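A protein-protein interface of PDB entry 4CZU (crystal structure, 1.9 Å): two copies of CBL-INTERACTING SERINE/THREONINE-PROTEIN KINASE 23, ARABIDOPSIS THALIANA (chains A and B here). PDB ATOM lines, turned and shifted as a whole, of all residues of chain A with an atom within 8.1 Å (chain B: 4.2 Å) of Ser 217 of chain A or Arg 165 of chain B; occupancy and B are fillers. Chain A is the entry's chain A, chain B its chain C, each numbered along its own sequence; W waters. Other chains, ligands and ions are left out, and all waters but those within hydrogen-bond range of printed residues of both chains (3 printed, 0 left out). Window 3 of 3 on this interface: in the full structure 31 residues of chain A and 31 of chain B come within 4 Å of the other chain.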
ATOM      1  N   ASN A 178      15.501 -25.287 -33.964  1.00  0.00           N
ATOM      2  CA  ASN A 178      15.682 -25.134 -32.520  1.00  0.00           C
ATOM      3  C   ASN A 178      16.379 -26.321 -31.864  1.00  0.00           C
ATOM      4  O   ASN A 178      17.012 -26.165 -30.817  1.00  0.00           O
ATOM      5  CB  ASN A 178      14.330 -24.862 -31.838  1.00  0.00           C
ATOM      6  CG  ASN A 178      13.553 -23.750 -32.514  1.00  0.00           C
ATOM      7  OD1 ASN A 178      13.021 -23.932 -33.609  1.00  0.00           O
ATOM      8  ND2 ASN A 178      13.471 -22.583 -31.857  1.00  0.00           N
ATOM      9  N   TYR A 211      10.541 -24.705 -21.493  1.00  0.00           N
ATOM     10  CA  TYR A 211      10.608 -23.957 -22.751  1.00  0.00           C
ATOM     11  C   TYR A 211      11.951 -24.158 -23.418  1.00  0.00           C
ATOM     12  O   TYR A 211      12.870 -24.736 -22.823  1.00  0.00           O
ATOM     13  CB  TYR A 211      10.349 -22.461 -22.528  1.00  0.00           C
ATOM     14  CG  TYR A 211      11.308 -21.810 -21.546  1.00  0.00           C
ATOM     15  CD1 TYR A 211      11.037 -21.814 -20.180  1.00  0.00           C
ATOM     16  CD2 TYR A 211      12.475 -21.192 -21.982  1.00  0.00           C
ATOM     17  CE1 TYR A 211      11.902 -21.220 -19.275  1.00  0.00           C
ATOM     18  CE2 TYR A 211      13.354 -20.597 -21.079  1.00  0.00           C
ATOM     19  CZ  TYR A 211      13.053 -20.605 -19.727  1.00  0.00           C
ATOM     20  OH  TYR A 211      13.911 -20.015 -18.822  1.00  0.00           O
ATOM     21  N   GLU A 215      14.956 -19.508 -28.929  1.00  0.00           N
ATOM     22  CA  GLU A 215      13.728 -19.309 -29.680  1.00  0.00           C
ATOM     23  C   GLU A 215      13.650 -17.851 -30.079  1.00  0.00           C
ATOM     24  O   GLU A 215      14.180 -16.989 -29.388  1.00  0.00           O
ATOM     25  CB  GLU A 215      12.500 -19.714 -28.851  1.00  0.00           C
ATOM     26  CG  GLU A 215      12.356 -18.960 -27.544  1.00  0.00           C
ATOM     27  CD  GLU A 215      11.166 -19.436 -26.713  1.00  0.00           C
ATOM     28  OE1 GLU A 215      10.211 -20.002 -27.296  1.00  0.00           O
ATOM     29  OE2 GLU A 215      11.188 -19.246 -25.475  1.00  0.00           O
ATOM     30  N   ASP A 216      13.016 -17.579 -31.216  1.00  0.00           N
ATOM     31  CA  ASP A 216      12.797 -16.197 -31.649  1.00  0.00           C
ATOM     32  C   ASP A 216      11.874 -16.245 -32.852  1.00  0.00           C
ATOM     33  O   ASP A 216      12.010 -17.140 -33.694  1.00  0.00           O
ATOM     34  CB  ASP A 216      14.127 -15.544 -32.063  1.00  0.00           C
ATOM     35  CG  ASP A 216      14.123 -14.023 -31.884  1.00  0.00           C
ATOM     36  OD1 ASP A 216      13.275 -13.339 -32.493  1.00  0.00           O
ATOM     37  OD2 ASP A 216      14.980 -13.513 -31.120  1.00  0.00           O
ATOM     38  N   SER A 217      10.945 -15.296 -32.941  1.00  0.00           N
ATOM     39  CA  SER A 217      10.063 -15.193 -34.100  1.00  0.00           C
ATOM     40  C   SER A 217      10.824 -14.691 -35.333  1.00  0.00           C
ATOM     41  O   SER A 217      10.408 -14.935 -36.472  1.00  0.00           O
ATOM     42  CB  SER A 217       8.891 -14.257 -33.801  1.00  0.00           C
ATOM     43  OG  SER A 217       9.357 -12.959 -33.473  1.00  0.00           O
ATOM     44  N   ASN A 218      11.933 -13.989 -35.095  1.00  0.00           N
ATOM     45  CA  ASN A 218      12.817 -13.506 -36.162  1.00  0.00           C
ATOM     46  C   ASN A 218      13.875 -14.559 -36.492  1.00  0.00           C
ATOM     47  O   ASN A 218      14.714 -14.891 -35.646  1.00  0.00           O
ATOM     48  CB  ASN A 218      13.488 -12.180 -35.739  1.00  0.00           C
ATOM     49  CG  ASN A 218      14.373 -11.590 -36.829  1.00  0.00           C
ATOM     50  OD1 ASN A 218      15.393 -12.169 -37.202  1.00  0.00           O
ATOM     51  ND2 ASN A 218      13.992 -10.415 -37.336  1.00  0.00           N
ATOM     52  N   LEU A 219      13.835 -15.086 -37.721  1.00  0.00           N
ATOM     53  CA  LEU A 219      14.697 -16.211 -38.121  1.00  0.00           C
ATOM     54  C   LEU A 219      16.192 -15.898 -38.029  1.00  0.00           C
ATOM     55  O   LEU A 219      16.991 -16.752 -37.642  1.00  0.00           O
ATOM     56  CB  LEU A 219      14.359 -16.666 -39.550  1.00  0.00           C
ATOM     57  CG  LEU A 219      13.528 -17.928 -39.819  1.00  0.00           C
ATOM     58  CD1 LEU A 219      12.787 -18.417 -38.588  1.00  0.00           C
ATOM     59  CD2 LEU A 219      12.552 -17.708 -40.988  1.00  0.00           C
ATOM     60  N   THR A 220      16.566 -14.678 -38.405  1.00  0.00           N
ATOM     61  CA  THR A 220      17.950 -14.230 -38.287  1.00  0.00           C
ATOM     62  C   THR A 220      18.428 -14.265 -36.831  1.00  0.00           C
ATOM     63  O   THR A 220      19.516 -14.748 -36.543  1.00  0.00           O
ATOM     64  CB  THR A 220      18.099 -12.780 -38.808  1.00  0.00           C
ATOM     65  OG1 THR A 220      17.653 -12.720 -40.166  1.00  0.00           O
ATOM     66  CG2 THR A 220      19.552 -12.329 -38.746  1.00  0.00           C
ATOM     67  N   SER A 221      17.619 -13.733 -35.920  1.00  0.00           N
ATOM     68  CA  SER A 221      17.974 -13.721 -34.503  1.00  0.00           C
ATOM     69  C   SER A 221      18.027 -15.144 -33.943  1.00  0.00           C
ATOM     70  O   SER A 221      18.881 -15.471 -33.114  1.00  0.00           O
ATOM     71  CB  SER A 221      16.974 -12.885 -33.703  1.00  0.00           C
ATOM     72  OG  SER A 221      16.839 -11.589 -34.272  1.00  0.00           O
ATOM     73  N   LEU A 222      17.113 -15.989 -34.402  1.00  0.00           N
ATOM     74  CA  LEU A 222      17.096 -17.387 -33.977  1.00  0.00           C
ATOM     75  C   LEU A 222      18.429 -18.083 -34.311  1.00  0.00           C
ATOM     76  O   LEU A 222      19.097 -18.619 -33.422  1.00  0.00           O
ATOM     77  CB  LEU A 222      15.920 -18.122 -34.631  1.00  0.00           C
ATOM     78  CG  LEU A 222      15.820 -19.614 -34.281  1.00  0.00           C
ATOM     79  CD1 LEU A 222      15.953 -19.859 -32.774  1.00  0.00           C
ATOM     80  CD2 LEU A 222      14.499 -20.184 -34.820  1.00  0.00           C
ATOM     81  N   LYS A 225      21.311 -16.742 -32.210  1.00  0.00           N
ATOM     82  CA  LYS A 225      21.303 -17.272 -30.849  1.00  0.00           C
ATOM     83  C   LYS A 225      21.893 -18.678 -30.812  1.00  0.00           C
ATOM     84  O   LYS A 225      22.642 -19.028 -29.900  1.00  0.00           O
ATOM     85  CB  LYS A 225      19.875 -17.322 -30.303  1.00  0.00           C
ATOM     86  CG  LYS A 225      19.317 -15.984 -29.832  1.00  0.00           C
ATOM     87  CD  LYS A 225      17.840 -16.120 -29.454  1.00  0.00           C
ATOM     88  CE  LYS A 225      17.276 -14.797 -28.945  1.00  0.00           C
ATOM     89  NZ  LYS A 225      15.844 -14.953 -28.575  1.00  0.00           N
ATOM     90  N   ASP B 136       2.999 -13.170 -37.183  1.00  0.00           N
ATOM     91  CA  ASP B 136       3.719 -14.402 -36.839  1.00  0.00           C
ATOM     92  C   ASP B 136       2.789 -15.602 -36.709  1.00  0.00           C
ATOM     93  O   ASP B 136       2.920 -16.400 -35.791  1.00  0.00           O
ATOM     94  CB  ASP B 136       4.514 -14.224 -35.544  1.00  0.00           C
ATOM     95  CG  ASP B 136       5.564 -15.313 -35.356  1.00  0.00           C
ATOM     96  OD1 ASP B 136       6.216 -15.705 -36.359  1.00  0.00           O
ATOM     97  OD2 ASP B 136       5.721 -15.796 -34.212  1.00  0.00           O
ATOM     98  N   SER B 158       1.292 -10.586 -30.144  1.00  0.00           N
ATOM     99  CA  SER B 158       2.445 -10.859 -31.000  1.00  0.00           C
ATOM    100  C   SER B 158       3.279  -9.599 -31.285  1.00  0.00           C
ATOM    101  O   SER B 158       4.439  -9.689 -31.692  1.00  0.00           O
ATOM    102  CB  SER B 158       1.994 -11.537 -32.305  1.00  0.00           C
ATOM    103  OG  SER B 158       1.251 -10.648 -33.134  1.00  0.00           O
ATOM    104  N   LEU B 160       4.210  -7.559 -28.937  1.00  0.00           N
ATOM    105  CA  LEU B 160       5.061  -7.281 -27.780  1.00  0.00           C
ATOM    106  C   LEU B 160       6.520  -7.643 -28.088  1.00  0.00           C
ATOM    107  O   LEU B 160       6.778  -8.474 -28.964  1.00  0.00           O
ATOM    108  CB  LEU B 160       4.545  -8.036 -26.552  1.00  0.00           C
ATOM    109  CG  LEU B 160       3.134  -7.632 -26.109  1.00  0.00           C
ATOM    110  CD1 LEU B 160       2.568  -8.646 -25.106  1.00  0.00           C
ATOM    111  CD2 LEU B 160       3.126  -6.229 -25.516  1.00  0.00           C
ATOM    112  N   PRO B 161       7.479  -7.008 -27.393  1.00  0.00           N
ATOM    113  CA  PRO B 161       8.898  -7.333 -27.603  1.00  0.00           C
ATOM    114  C   PRO B 161       9.235  -8.807 -27.346  1.00  0.00           C
ATOM    115  O   PRO B 161       8.632  -9.438 -26.478  1.00  0.00           O
ATOM    116  CB  PRO B 161       9.630  -6.431 -26.589  1.00  0.00           C
ATOM    117  CG  PRO B 161       8.578  -5.931 -25.668  1.00  0.00           C
ATOM    118  CD  PRO B 161       7.311  -5.889 -26.451  1.00  0.00           C
ATOM    119  N   GLN B 162      10.202  -9.328 -28.097  1.00  0.00           N
ATOM    120  CA  GLN B 162      10.604 -10.733 -28.037  1.00  0.00           C
ATOM    121  C   GLN B 162      10.864 -11.260 -26.629  1.00  0.00           C
ATOM    122  O   GLN B 162      10.448 -12.367 -26.284  1.00  0.00           O
ATOM    123  CB  GLN B 162      11.852 -10.961 -28.900  1.00  0.00           C
ATOM    124  CG  GLN B 162      12.386 -12.385 -28.871  1.00  0.00           C
ATOM    125  CD  GLN B 162      11.346 -13.408 -29.281  1.00  0.00           C
ATOM    126  OE1 GLN B 162      10.463 -13.130 -30.103  1.00  0.00           O
ATOM    127  NE2 GLN B 162      11.440 -14.600 -28.711  1.00  0.00           N
ATOM    128  N   GLN B 163      11.559 -10.471 -25.820  1.00  0.00           N
ATOM    129  CA  GLN B 163      11.937 -10.902 -24.477  1.00  0.00           C
ATOM    130  C   GLN B 163      10.748 -11.113 -23.553  1.00  0.00           C
ATOM    131  O   GLN B 163      10.876 -11.735 -22.504  1.00  0.00           O
ATOM    132  CB  GLN B 163      12.876  -9.881 -23.839  1.00  0.00           C
ATOM    133  CG  GLN B 163      14.307  -9.990 -24.300  1.00  0.00           C
ATOM    134  CD  GLN B 163      15.227  -9.095 -23.501  1.00  0.00           C
ATOM    135  OE1 GLN B 163      15.008  -7.886 -23.403  1.00  0.00           O
ATOM    136  NE2 GLN B 163      16.260  -9.687 -22.910  1.00  0.00           N
ATOM    137  N   VAL B 164       9.600 -10.581 -23.942  1.00  0.00           N
ATOM    138  CA  VAL B 164       8.378 -10.712 -23.166  1.00  0.00           C
ATOM    139  C   VAL B 164       7.466 -11.773 -23.806  1.00  0.00           C
ATOM    140  O   VAL B 164       6.499 -12.248 -23.199  1.00  0.00           O
ATOM    141  CB  VAL B 164       7.708  -9.310 -23.014  1.00  0.00           C
ATOM    142  CG1 VAL B 164       6.334  -9.239 -23.669  1.00  0.00           C
ATOM    143  CG2 VAL B 164       7.685  -8.874 -21.559  1.00  0.00           C
ATOM    144  N   ARG B 165       7.798 -12.161 -25.033  1.00  0.00           N
ATOM    145  CA  ARG B 165       7.106 -13.264 -25.688  1.00  0.00           C
ATOM    146  C   ARG B 165       7.696 -14.595 -25.221  1.00  0.00           C
ATOM    147  O   ARG B 165       7.092 -15.652 -25.399  1.00  0.00           O
ATOM    148  CB  ARG B 165       7.169 -13.128 -27.216  1.00  0.00           C
ATOM    149  CG  ARG B 165       6.401 -11.933 -27.767  1.00  0.00           C
ATOM    150  CD  ARG B 165       6.434 -11.875 -29.292  1.00  0.00           C
ATOM    151  NE  ARG B 165       5.659 -12.949 -29.912  1.00  0.00           N
ATOM    152  CZ  ARG B 165       5.566 -13.137 -31.226  1.00  0.00           C
ATOM    153  NH1 ARG B 165       6.198 -12.324 -32.066  1.00  0.00           N
ATOM    154  NH2 ARG B 165       4.841 -14.137 -31.706  1.00  0.00           N
ATOM    155  N   GLU B 166       8.879 -14.538 -24.612  1.00  0.00           N
ATOM    156  CA  GLU B 166       9.487 -15.710 -23.988  1.00  0.00           C
ATOM    157  C   GLU B 166       8.908 -15.844 -22.579  1.00  0.00           C
ATOM    158  O   GLU B 166       9.459 -15.334 -21.600  1.00  0.00           O
ATOM    159  CB  GLU B 166      11.013 -15.589 -23.970  1.00  0.00           C
ATOM    160  CG  GLU B 166      11.604 -15.605 -25.380  1.00  0.00           C
ATOM    161  CD  GLU B 166      13.087 -15.269 -25.434  1.00  0.00           C
ATOM    162  OE1 GLU B 166      13.702 -15.070 -24.366  1.00  0.00           O
ATOM    163  OE2 GLU B 166      13.643 -15.205 -26.561  1.00  0.00           O
ATOM    164  N   ASP B 167       7.773 -16.529 -22.498  1.00  0.00           N
ATOM    165  CA  ASP B 167       6.923 -16.484 -21.310  1.00  0.00           C
ATOM    166  C   ASP B 167       6.878 -17.803 -20.536  1.00  0.00           C
ATOM    167  O   ASP B 167       5.966 -18.031 -19.734  1.00  0.00           O
ATOM    168  CB  ASP B 167       5.514 -16.096 -21.739  1.00  0.00           C
ATOM    169  CG  ASP B 167       4.991 -16.959 -22.883  1.00  0.00           C
ATOM    170  OD1 ASP B 167       5.657 -17.959 -23.260  1.00  0.00           O
ATOM    171  OD2 ASP B 167       3.896 -16.651 -23.401  1.00  0.00           O
ATOM    172  N   HIS B 171       7.240 -23.256 -27.262  1.00  0.00           N
ATOM    173  CA  HIS B 171       6.837 -22.779 -28.587  1.00  0.00           C
ATOM    174  C   HIS B 171       7.670 -23.379 -29.709  1.00  0.00           C
ATOM    175  O   HIS B 171       8.628 -22.759 -30.166  1.00  0.00           O
ATOM    176  CB  HIS B 171       7.010 -21.261 -28.726  1.00  0.00           C
ATOM    177  CG  HIS B 171       6.378 -20.472 -27.630  1.00  0.00           C
ATOM    178  ND1 HIS B 171       5.013 -20.305 -27.526  1.00  0.00           N
ATOM    179  CD2 HIS B 171       6.927 -19.790 -26.598  1.00  0.00           C
ATOM    180  CE1 HIS B 171       4.747 -19.563 -26.463  1.00  0.00           C
ATOM    181  NE2 HIS B 171       5.889 -19.241 -25.879  1.00  0.00           N
HETATM  182  O   HOH W   1       9.550 -22.285 -26.013  1.00  0.00           O
HETATM  183  O   HOH W   2      15.644 -17.761 -26.582  1.00  0.00           O
HETATM  184  O   HOH W   3       9.010 -19.209 -23.912  1.00  0.00           O
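Printed residues of chain A within 4 Å of Arg 165 of chain B: Ser 217 (3.5 Å). Printed residues of chain A within 4 Å of Asp 136 of chain B: Ser 217. Of the printed residues of chain A, His 171 of chain B touches Glu 215. Of the printed residues of chain B, Lys 225 of chain A touches Glu 166. Printed residues of chain B within 4 Å of Asp 216 of chain A: Gln 162. The nearest printed residue of chain B that does not touch Ser 217 of chain A is Ser 158 of chain B (6.2 Å).
No position is printed for both chains.
The side-chain amino group (NZ) of Lys 225 of chain A is in salt-bridge range of the side-chain carboxylate (OE2) of Glu 166 of chain B (3.0 Å). The backbone carbonyl oxygen (O) of Glu 215 of chain A lies close to the side-chain carboxylate (OE2) of Glu 166 of chain B, at 3.4 Å.
Water W3 bridges OE2 of Glu 215 of chain A and N of Asp 167 of chain B. Water W1 lies within hydrogen-bond range of the side-chain carboxylate (OE1) of Glu 215 of chain A and the backbone NH (N) of His 171 of chain B. Water W2 lies within hydrogen-bond range of the backbone NH (N) of Glu 215 of chain A (3.0 Å), the side-chain carboxylate (OE2) of Glu 166 of chain B (3.2 Å) and the side-chain amino group (NZ) of Lys 225 of chain A (3.4 Å).
Gln 162 of chain B touches Glu 215 of chain A. His 171 of chain B touches Glu 215 of chain A. Asp 216 of chain A touches Gln 162 of chain B (CA to NE2, 3.6 Å). Ser 217 of chain A touches Asp 136 of chain B. Ser 217 of chain A touches Gln 162 of chain B. Ser 217 of chain A touches Arg 165 of chain B (OG to NH1, 3.5 Å).
O of Glu 215 of chain A sits at hydrogen-bond distance from NZ of Lys 225 of chain A (2.8 Å). N of Asn 218 of chain A lies within hydrogen-bond range of OD1 of Asp 216 of chain A. The side-chain carboxylate of Asp 216 of chain A is in salt-bridge range of the side-chain amino group of Lys 225 of chain A (3.0 Å). The guanidinium group of Arg 165 of chain B is in salt-bridge range of the side-chain carboxylate of Asp 136 of chain B. The guanidinium group (NH1) of Arg 165 of chain B lies within hydrogen-bond range of the backbone carbonyl oxygen (O) of Ser 158 of chain B, 3.2 Å away. The side-chain carboxylate (OE2) of Glu 166 of chain B lies within hydrogen-bond range of the side-chain amide nitrogen (NE2) of Gln 162 of chain B.
Of the 11 printed residues of chain B, 5 touch a printed residue of chain A. Hydrophobic or aromatic side chains of chain B that line the printed part of chain A: His 171. Printed residues of chain A that touch a printed residue of chain B: Glu 215, Asp 216, Ser 217 and Lys 225.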
